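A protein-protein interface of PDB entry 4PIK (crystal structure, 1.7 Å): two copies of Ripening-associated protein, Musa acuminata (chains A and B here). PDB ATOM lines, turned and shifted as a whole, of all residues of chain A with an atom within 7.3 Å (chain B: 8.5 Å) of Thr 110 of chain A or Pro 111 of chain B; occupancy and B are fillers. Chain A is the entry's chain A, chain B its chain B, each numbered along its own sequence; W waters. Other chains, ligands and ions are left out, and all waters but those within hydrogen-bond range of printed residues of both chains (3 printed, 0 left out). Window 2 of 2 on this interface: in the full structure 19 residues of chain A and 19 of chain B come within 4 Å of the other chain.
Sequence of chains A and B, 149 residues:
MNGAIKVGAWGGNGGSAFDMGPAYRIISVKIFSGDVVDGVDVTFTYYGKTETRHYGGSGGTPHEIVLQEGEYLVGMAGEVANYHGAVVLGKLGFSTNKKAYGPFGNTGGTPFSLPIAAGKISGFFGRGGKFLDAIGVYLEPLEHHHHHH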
ATOM      1  N   TRP A  10     -34.043  18.534  18.117  1.00  0.00           N
ATOM      2  CA  TRP A  10     -33.084  17.478  18.403  1.00  0.00           C
ATOM      3  C   TRP A  10     -33.886  16.273  18.818  1.00  0.00           C
ATOM      4  O   TRP A  10     -34.814  16.405  19.624  1.00  0.00           O
ATOM      5  CB  TRP A  10     -32.101  17.893  19.556  1.00  0.00           C
ATOM      6  CG  TRP A  10     -31.167  19.010  19.195  1.00  0.00           C
ATOM      7  CD1 TRP A  10     -29.951  18.889  18.587  1.00  0.00           C
ATOM      8  CD2 TRP A  10     -31.395  20.425  19.370  1.00  0.00           C
ATOM      9  NE1 TRP A  10     -29.408  20.144  18.358  1.00  0.00           N
ATOM     10  CE2 TRP A  10     -30.257  21.099  18.862  1.00  0.00           C
ATOM     11  CE3 TRP A  10     -32.481  21.186  19.838  1.00  0.00           C
ATOM     12  CZ2 TRP A  10     -30.117  22.495  18.917  1.00  0.00           C
ATOM     13  CZ3 TRP A  10     -32.351  22.580  19.885  1.00  0.00           C
ATOM     14  CH2 TRP A  10     -31.193  23.218  19.408  1.00  0.00           C
ATOM     15  N   GLY A  78     -29.131  18.338  26.240  1.00  0.00           N
ATOM     16  CA  GLY A  78     -29.606  16.998  26.543  1.00  0.00           C
ATOM     17  C   GLY A  78     -28.865  15.966  25.744  1.00  0.00           C
ATOM     18  O   GLY A  78     -27.795  16.247  25.238  1.00  0.00           O
ATOM     19  N   GLU A  79     -29.440  14.758  25.671  1.00  0.00           N
ATOM     20  CA  GLU A  79     -28.854  13.640  24.936  1.00  0.00           C
ATOM     21  C   GLU A  79     -29.946  12.954  24.169  1.00  0.00           C
ATOM     22  O   GLU A  79     -31.063  12.764  24.683  1.00  0.00           O
ATOM     23  CB  GLU A  79     -28.140  12.652  25.877  1.00  0.00           C
ATOM     24  CG  GLU A  79     -26.976  13.371  26.560  1.00  0.00           C
ATOM     25  CD  GLU A  79     -25.880  12.588  27.248  1.00  0.00           C
ATOM     26  OE1 GLU A  79     -25.952  11.340  27.277  1.00  0.00           O
ATOM     27  OE2 GLU A  79     -24.982  13.232  27.836  1.00  0.00           O
ATOM     28  N   VAL A  80     -29.659  12.660  22.900  1.00  0.00           N
ATOM     29  CA  VAL A  80     -30.585  11.935  22.023  1.00  0.00           C
ATOM     30  C   VAL A  80     -30.211  10.469  22.151  1.00  0.00           C
ATOM     31  O   VAL A  80     -29.098  10.086  21.775  1.00  0.00           O
ATOM     32  CB  VAL A  80     -30.507  12.450  20.580  1.00  0.00           C
ATOM     33  CG1 VAL A  80     -31.269  11.511  19.642  1.00  0.00           C
ATOM     34  CG2 VAL A  80     -31.053  13.881  20.506  1.00  0.00           C
ATOM     35  N   ALA A  81     -31.128   9.661  22.684  1.00  0.00           N
ATOM     36  CA  ALA A  81     -30.828   8.285  23.012  1.00  0.00           C
ATOM     37  C   ALA A  81     -31.586   7.276  22.208  1.00  0.00           C
ATOM     38  O   ALA A  81     -32.666   7.543  21.720  1.00  0.00           O
ATOM     39  CB  ALA A  81     -31.160   8.050  24.481  1.00  0.00           C
ATOM     40  N   ASN A  82     -31.056   6.056  22.202  1.00  0.00           N
ATOM     41  CA  ASN A  82     -31.721   4.919  21.604  1.00  0.00           C
ATOM     42  C   ASN A  82     -32.346   4.180  22.746  1.00  0.00           C
ATOM     43  O   ASN A  82     -31.633   3.812  23.686  1.00  0.00           O
ATOM     44  CB  ASN A  82     -30.672   4.074  20.884  1.00  0.00           C
ATOM     45  CG  ASN A  82     -31.242   3.142  19.840  1.00  0.00           C
ATOM     46  OD1 ASN A  82     -32.453   3.190  19.451  1.00  0.00           O
ATOM     47  ND2 ASN A  82     -30.382   2.219  19.437  1.00  0.00           N
ATOM     48  N   LEU A  89     -35.546  11.715  23.358  1.00  0.00           N
ATOM     49  CA  LEU A  89     -34.688  12.443  24.301  1.00  0.00           C
ATOM     50  C   LEU A  89     -34.399  11.541  25.500  1.00  0.00           C
ATOM     51  O   LEU A  89     -35.320  11.210  26.224  1.00  0.00           O
ATOM     52  CB  LEU A  89     -35.409  13.724  24.763  1.00  0.00           C
ATOM     53  CG  LEU A  89     -35.242  14.974  23.868  1.00  0.00           C
ATOM     54  CD1 LEU A  89     -33.808  15.483  23.901  1.00  0.00           C
ATOM     55  CD2 LEU A  89     -35.625  14.733  22.470  1.00  0.00           C
ATOM     56  N   THR A 107     -30.859   8.088  30.212  1.00  0.00           N
ATOM     57  CA  THR A 107     -30.265   7.322  29.119  1.00  0.00           C
ATOM     58  C   THR A 107     -29.358   8.207  28.284  1.00  0.00           C
ATOM     59  O   THR A 107     -29.790   9.218  27.709  1.00  0.00           O
ATOM     60  CB  THR A 107     -31.344   6.670  28.254  1.00  0.00           C
ATOM     61  OG1 THR A 107     -32.191   5.867  29.078  1.00  0.00           O
ATOM     62  CG2 THR A 107     -30.698   5.738  27.190  1.00  0.00           C
ATOM     63  N   GLY A 108     -28.102   7.797  28.208  1.00  0.00           N
ATOM     64  CA  GLY A 108     -27.106   8.527  27.452  1.00  0.00           C
ATOM     65  C   GLY A 108     -27.255   8.314  25.958  1.00  0.00           C
ATOM     66  O   GLY A 108     -27.837   7.317  25.496  1.00  0.00           O
ATOM     67  N   GLY A 109     -26.718   9.240  25.215  1.00  0.00           N
ATOM     68  CA  GLY A 109     -26.719   9.174  23.768  1.00  0.00           C
ATOM     69  C   GLY A 109     -25.877  10.271  23.192  1.00  0.00           C
ATOM     70  O   GLY A 109     -24.838  10.618  23.764  1.00  0.00           O
ATOM     71  N   THR A 110     -26.326  10.818  22.074  1.00  0.00           N
ATOM     72  CA  THR A 110     -25.604  11.902  21.399  1.00  0.00           C
ATOM     73  C   THR A 110     -25.951  13.226  22.070  1.00  0.00           C
ATOM     74  O   THR A 110     -27.106  13.671  21.994  1.00  0.00           O
ATOM     75  CB  THR A 110     -25.941  11.933  19.904  1.00  0.00           C
ATOM     76  OG1 THR A 110     -25.729  10.626  19.367  1.00  0.00           O
ATOM     77  CG2 THR A 110     -25.070  12.943  19.131  1.00  0.00           C
ATOM     78  N   PRO A 111     -24.966  13.869  22.697  1.00  0.00           N
ATOM     79  CA  PRO A 111     -25.260  15.160  23.344  1.00  0.00           C
ATOM     80  C   PRO A 111     -25.592  16.281  22.375  1.00  0.00           C
ATOM     81  O   PRO A 111     -25.125  16.339  21.238  1.00  0.00           O
ATOM     82  CB  PRO A 111     -23.978  15.516  24.105  1.00  0.00           C
ATOM     83  CG  PRO A 111     -22.938  14.620  23.607  1.00  0.00           C
ATOM     84  CD  PRO A 111     -23.567  13.440  22.919  1.00  0.00           C
ATOM     85  N   PHE A 112     -26.375  17.219  22.882  1.00  0.00           N
ATOM     86  CA  PHE A 112     -26.646  18.481  22.208  1.00  0.00           C
ATOM     87  C   PHE A 112     -26.686  19.559  23.264  1.00  0.00           C
ATOM     88  O   PHE A 112     -26.924  19.292  24.455  1.00  0.00           O
ATOM     89  CB  PHE A 112     -27.929  18.522  21.342  1.00  0.00           C
ATOM     90  CG  PHE A 112     -29.219  18.494  22.129  1.00  0.00           C
ATOM     91  CD1 PHE A 112     -29.770  17.292  22.538  1.00  0.00           C
ATOM     92  CD2 PHE A 112     -29.886  19.679  22.450  1.00  0.00           C
ATOM     93  CE1 PHE A 112     -30.949  17.261  23.277  1.00  0.00           C
ATOM     94  CE2 PHE A 112     -31.049  19.652  23.229  1.00  0.00           C
ATOM     95  CZ  PHE A 112     -31.602  18.442  23.589  1.00  0.00           C
ATOM     96  N   SER A 113     -26.478  20.798  22.802  1.00  0.00           N
ATOM     97  CA  SER A 113     -26.462  21.918  23.729  1.00  0.00           C
ATOM     98  C   SER A 113     -26.797  23.160  22.972  1.00  0.00           C
ATOM     99  O   SER A 113     -26.354  23.350  21.831  1.00  0.00           O
ATOM    100  CB  SER A 113     -25.100  22.059  24.396  1.00  0.00           C
ATOM    101  OG  SER A 113     -24.075  22.190  23.419  1.00  0.00           O
ATOM    102  N   TRP B  10     -19.926  27.409  20.988  1.00  0.00           N
ATOM    103  CA  TRP B  10     -19.543  26.034  21.295  1.00  0.00           C
ATOM    104  C   TRP B  10     -18.054  25.973  21.231  1.00  0.00           C
ATOM    105  O   TRP B  10     -17.490  26.532  20.291  1.00  0.00           O
ATOM    106  CB  TRP B  10     -20.151  25.072  20.281  1.00  0.00           C
ATOM    107  CG  TRP B  10     -21.634  24.924  20.450  1.00  0.00           C
ATOM    108  CD1 TRP B  10     -22.287  24.045  21.270  1.00  0.00           C
ATOM    109  CD2 TRP B  10     -22.647  25.678  19.773  1.00  0.00           C
ATOM    110  NE1 TRP B  10     -23.646  24.190  21.129  1.00  0.00           N
ATOM    111  CE2 TRP B  10     -23.897  25.223  20.255  1.00  0.00           C
ATOM    112  CE3 TRP B  10     -22.621  26.713  18.815  1.00  0.00           C
ATOM    113  CZ2 TRP B  10     -25.110  25.709  19.751  1.00  0.00           C
ATOM    114  CZ3 TRP B  10     -23.821  27.261  18.384  1.00  0.00           C
ATOM    115  CH2 TRP B  10     -25.048  26.740  18.823  1.00  0.00           C
ATOM    116  N   ALA B  77     -22.693  22.533  12.611  1.00  0.00           N
ATOM    117  CA  ALA B  77     -22.516  21.387  13.511  1.00  0.00           C
ATOM    118  C   ALA B  77     -21.054  21.057  13.615  1.00  0.00           C
ATOM    119  O   ALA B  77     -20.252  21.552  12.841  1.00  0.00           O
ATOM    120  CB  ALA B  77     -23.308  20.177  13.002  1.00  0.00           C
ATOM    121  N   GLY B  78     -20.696  20.245  14.578  1.00  0.00           N
ATOM    122  CA  GLY B  78     -19.281  19.905  14.705  1.00  0.00           C
ATOM    123  C   GLY B  78     -19.000  19.161  15.969  1.00  0.00           C
ATOM    124  O   GLY B  78     -19.905  18.525  16.525  1.00  0.00           O
ATOM    125  N   GLU B  79     -17.717  19.189  16.386  1.00  0.00           N
ATOM    126  CA  GLU B  79     -17.230  18.511  17.589  1.00  0.00           C
ATOM    127  C   GLU B  79     -16.327  19.423  18.345  1.00  0.00           C
ATOM    128  O   GLU B  79     -15.473  20.095  17.738  1.00  0.00           O
ATOM    129  CB  GLU B  79     -16.418  17.240  17.232  1.00  0.00           C
ATOM    130  CG  GLU B  79     -17.174  16.233  16.387  1.00  0.00           C
ATOM    131  CD  GLU B  79     -17.858  15.134  17.167  1.00  0.00           C
ATOM    132  OE1 GLU B  79     -17.560  14.976  18.375  1.00  0.00           O
ATOM    133  OE2 GLU B  79     -18.670  14.403  16.553  1.00  0.00           O
ATOM    134  N   VAL B  80     -16.487  19.426  19.658  1.00  0.00           N
ATOM    135  CA  VAL B  80     -15.619  20.133  20.602  1.00  0.00           C
ATOM    136  C   VAL B  80     -14.628  19.095  21.099  1.00  0.00           C
ATOM    137  O   VAL B  80     -15.040  18.088  21.693  1.00  0.00           O
ATOM    138  CB  VAL B  80     -16.370  20.824  21.760  1.00  0.00           C
ATOM    139  CG1 VAL B  80     -15.378  21.437  22.735  1.00  0.00           C
ATOM    140  CG2 VAL B  80     -17.350  21.889  21.239  1.00  0.00           C
ATOM    141  N   ALA B  81     -13.339  19.343  20.877  1.00  0.00           N
ATOM    142  CA  ALA B  81     -12.295  18.361  21.192  1.00  0.00           C
ATOM    143  C   ALA B  81     -11.242  18.867  22.129  1.00  0.00           C
ATOM    144  O   ALA B  81     -10.985  20.063  22.205  1.00  0.00           O
ATOM    145  CB  ALA B  81     -11.633  17.935  19.901  1.00  0.00           C
ATOM    146  N   LYS B  91     -14.015  19.575  14.762  1.00  0.00           N
ATOM    147  CA  LYS B  91     -14.667  19.485  13.468  1.00  0.00           C
ATOM    148  C   LYS B  91     -15.689  20.600  13.374  1.00  0.00           C
ATOM    149  O   LYS B  91     -16.271  20.978  14.393  1.00  0.00           O
ATOM    150  CB  LYS B  91     -15.397  18.134  13.258  1.00  0.00           C
ATOM    151  CG  LYS B  91     -14.525  16.887  13.395  1.00  0.00           C
ATOM    152  CD  LYS B  91     -15.320  15.665  12.956  1.00  0.00           C
ATOM    153  CE  LYS B  91     -14.462  14.430  13.068  1.00  0.00           C
ATOM    154  NZ  LYS B  91     -15.236  13.217  12.701  1.00  0.00           N
ATOM    155  N   THR B 107     -10.780  15.569  14.463  1.00  0.00           N
ATOM    156  CA  THR B 107     -10.716  15.186  15.867  1.00  0.00           C
ATOM    157  C   THR B 107     -12.116  15.205  16.462  1.00  0.00           C
ATOM    158  O   THR B 107     -12.782  16.247  16.474  1.00  0.00           O
ATOM    159  CB  THR B 107      -9.720  16.036  16.691  1.00  0.00           C
ATOM    160  OG1 THR B 107      -8.434  16.047  16.052  1.00  0.00           O
ATOM    161  CG2 THR B 107      -9.556  15.502  18.136  1.00  0.00           C
ATOM    162  N   GLY B 108     -12.546  14.047  16.954  1.00  0.00           N
ATOM    163  CA  GLY B 108     -13.847  13.925  17.587  1.00  0.00           C
ATOM    164  C   GLY B 108     -13.771  14.381  19.022  1.00  0.00           C
ATOM    165  O   GLY B 108     -12.680  14.600  19.563  1.00  0.00           O
ATOM    166  N   GLY B 109     -14.930  14.507  19.644  1.00  0.00           N
ATOM    167  CA  GLY B 109     -15.032  14.875  21.041  1.00  0.00           C
ATOM    168  C   GLY B 109     -16.482  14.928  21.461  1.00  0.00           C
ATOM    169  O   GLY B 109     -17.172  13.899  21.451  1.00  0.00           O
ATOM    170  N   THR B 110     -16.934  16.100  21.878  1.00  0.00           N
ATOM    171  CA  THR B 110     -18.327  16.276  22.291  1.00  0.00           C
ATOM    172  C   THR B 110     -19.066  16.874  21.095  1.00  0.00           C
ATOM    173  O   THR B 110     -18.775  18.017  20.723  1.00  0.00           O
ATOM    174  CB  THR B 110     -18.438  17.124  23.561  1.00  0.00           C
ATOM    175  OG1 THR B 110     -17.675  16.505  24.609  1.00  0.00           O
ATOM    176  CG2 THR B 110     -19.894  17.318  24.027  1.00  0.00           C
ATOM    177  N   PRO B 111     -20.010  16.155  20.461  1.00  0.00           N
ATOM    178  CA  PRO B 111     -20.692  16.759  19.313  1.00  0.00           C
ATOM    179  C   PRO B 111     -21.630  17.893  19.700  1.00  0.00           C
ATOM    180  O   PRO B 111     -22.165  17.918  20.806  1.00  0.00           O
ATOM    181  CB  PRO B 111     -21.511  15.604  18.727  1.00  0.00           C
ATOM    182  CG  PRO B 111     -21.713  14.669  19.863  1.00  0.00           C
ATOM    183  CD  PRO B 111     -20.466  14.760  20.701  1.00  0.00           C
ATOM    184  N   PHE B 112     -21.855  18.807  18.748  1.00  0.00           N
ATOM    185  CA  PHE B 112     -22.886  19.832  18.858  1.00  0.00           C
ATOM    186  C   PHE B 112     -23.547  19.934  17.530  1.00  0.00           C
ATOM    187  O   PHE B 112     -22.955  19.589  16.490  1.00  0.00           O
ATOM    188  CB  PHE B 112     -22.372  21.195  19.328  1.00  0.00           C
ATOM    189  CG  PHE B 112     -21.482  21.911  18.352  1.00  0.00           C
ATOM    190  CD1 PHE B 112     -20.119  21.610  18.272  1.00  0.00           C
ATOM    191  CD2 PHE B 112     -22.005  22.868  17.485  1.00  0.00           C
ATOM    192  CE1 PHE B 112     -19.283  22.311  17.387  1.00  0.00           C
ATOM    193  CE2 PHE B 112     -21.185  23.508  16.552  1.00  0.00           C
ATOM    194  CZ  PHE B 112     -19.832  23.241  16.515  1.00  0.00           C
ATOM    195  N   SER B 113     -24.783  20.437  17.533  1.00  0.00           N
ATOM    196  CA  SER B 113     -25.517  20.583  16.297  1.00  0.00           C
ATOM    197  C   SER B 113     -26.499  21.685  16.420  1.00  0.00           C
ATOM    198  O   SER B 113     -27.147  21.813  17.459  1.00  0.00           O
ATOM    199  CB  SER B 113     -26.221  19.286  15.908  1.00  0.00           C
ATOM    200  OG  SER B 113     -26.977  18.803  17.014  1.00  0.00           O
ATOM    201  N   LEU B 114     -26.598  22.494  15.360  1.00  0.00           N
ATOM    202  CA  LEU B 114     -27.546  23.592  15.324  1.00  0.00           C
ATOM    203  C   LEU B 114     -28.399  23.508  14.081  1.00  0.00           C
ATOM    204  O   LEU B 114     -28.125  24.174  13.074  1.00  0.00           O
ATOM    205  CB  LEU B 114     -26.877  24.984  15.460  1.00  0.00           C
ATOM    206  CG  LEU B 114     -27.829  26.195  15.482  1.00  0.00           C
ATOM    207  CD1 LEU B 114     -28.630  26.273  16.808  1.00  0.00           C
ATOM    208  CD2 LEU B 114     -27.058  27.476  15.195  1.00  0.00           C
HETATM  209  O   HOH W   1     -25.583  17.126  18.573  1.00  0.00           O
HETATM  210  O   HOH W   2     -23.015  19.613  22.801  1.00  0.00           O
HETATM  211  O   HOH W   3     -26.093  21.356  19.902  1.00  0.00           O
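NE1 of Trp 10 of chain A is in hydrogen-bond range of O of Ser 113 of chain B, 3.0 Å away.
The backbone carbonyl oxygen (O) of Ser 113 of chain A is in hydrogen-bond range of the indole nitrogen (NE1) of Trp 10 of chain B.
O of Pro 111 of chain B lies close to O of Pro 111 of chain A, at 3.4 Å.
The backbone NH (N) of Thr 110 of chain A is in hydrogen-bond range of the backbone carbonyl oxygen (O) of Val 80 of chain A.
Among the printed residues, pairs that only touch across the chains: Thr 110 of chain A with Pro 111 of chain B.
Pro 111 of chain B touches just these residues of chain A: Thr 110 (3.8 Å) and Pro 111 (3.4 Å).
Gly 109 of chain A touches none of the printed residues of chain B.
Pro 111 of chain A touches one residue of chain B.
Printed residues of chain B within 4 Å of Ser 113 of chain A: Trp 10.
Of the printed residues of chain B, Trp 10 of chain A touches Ser 113 (3.0 Å).
Of the printed residues of chain A, Ser 113 of chain B touches Trp 10.
Phe 112 of chain A touches none of the printed residues of chain B.
Ala 77 of chain B touches none of the printed residues of chain A.
The nearest residue of chain B that does not touch Thr 110 of chain A is Ser 113 of chain B (6.5 Å).
The nearest printed residue of chain B that does not touch Ser 113 of chain A is Phe 112 of chain B (4.5 Å).
Hydrophobic or aromatic side chains of chain A within 4 Å of the printed part of chain B: Trp 10 and Pro 111.
Among the printed residues, no Asp or Glu carboxylate lies within 4 Å of a Lys or Arg side-chain nitrogen of the other chain.
Trp 10 of chain A touches Ser 113 of chain B, and with the chains exchanged Ser 113 of chain A touches Trp 10 of chain B.
Thr 110 of chain A touches Pro 111 of chain B, but with the chains exchanged Pro 111 of chain A does not touch Thr 110 of chain B (4.1 Å).
Pro 111 of chain B touches its own counterpart, Pro 111 of chain A.
Positions printed for both chains: 10, 78, 79, 80, 81, 107, 108, 109, 110, 111, 112 and 113.
Of the 4 pairs that touch across the chains among the printed residues, 3 have their exchanged pair printed and touching as well.
Water W1 bridges the side-chain hydroxyl (OG) of Ser 113 of chain B (2.7 Å) and the backbone carbonyl oxygen (O) of Pro 111 of chain A (2.8 Å).
Water W3 bridges O of Ser 113 of chain B and O of Ser 113 of chain A.
Water W2 bridges the backbone carbonyl oxygen (O) of Pro 111 of chain B (2.8 Å) and the side-chain hydroxyl (OG) of Ser 113 of chain A (2.9 Å).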
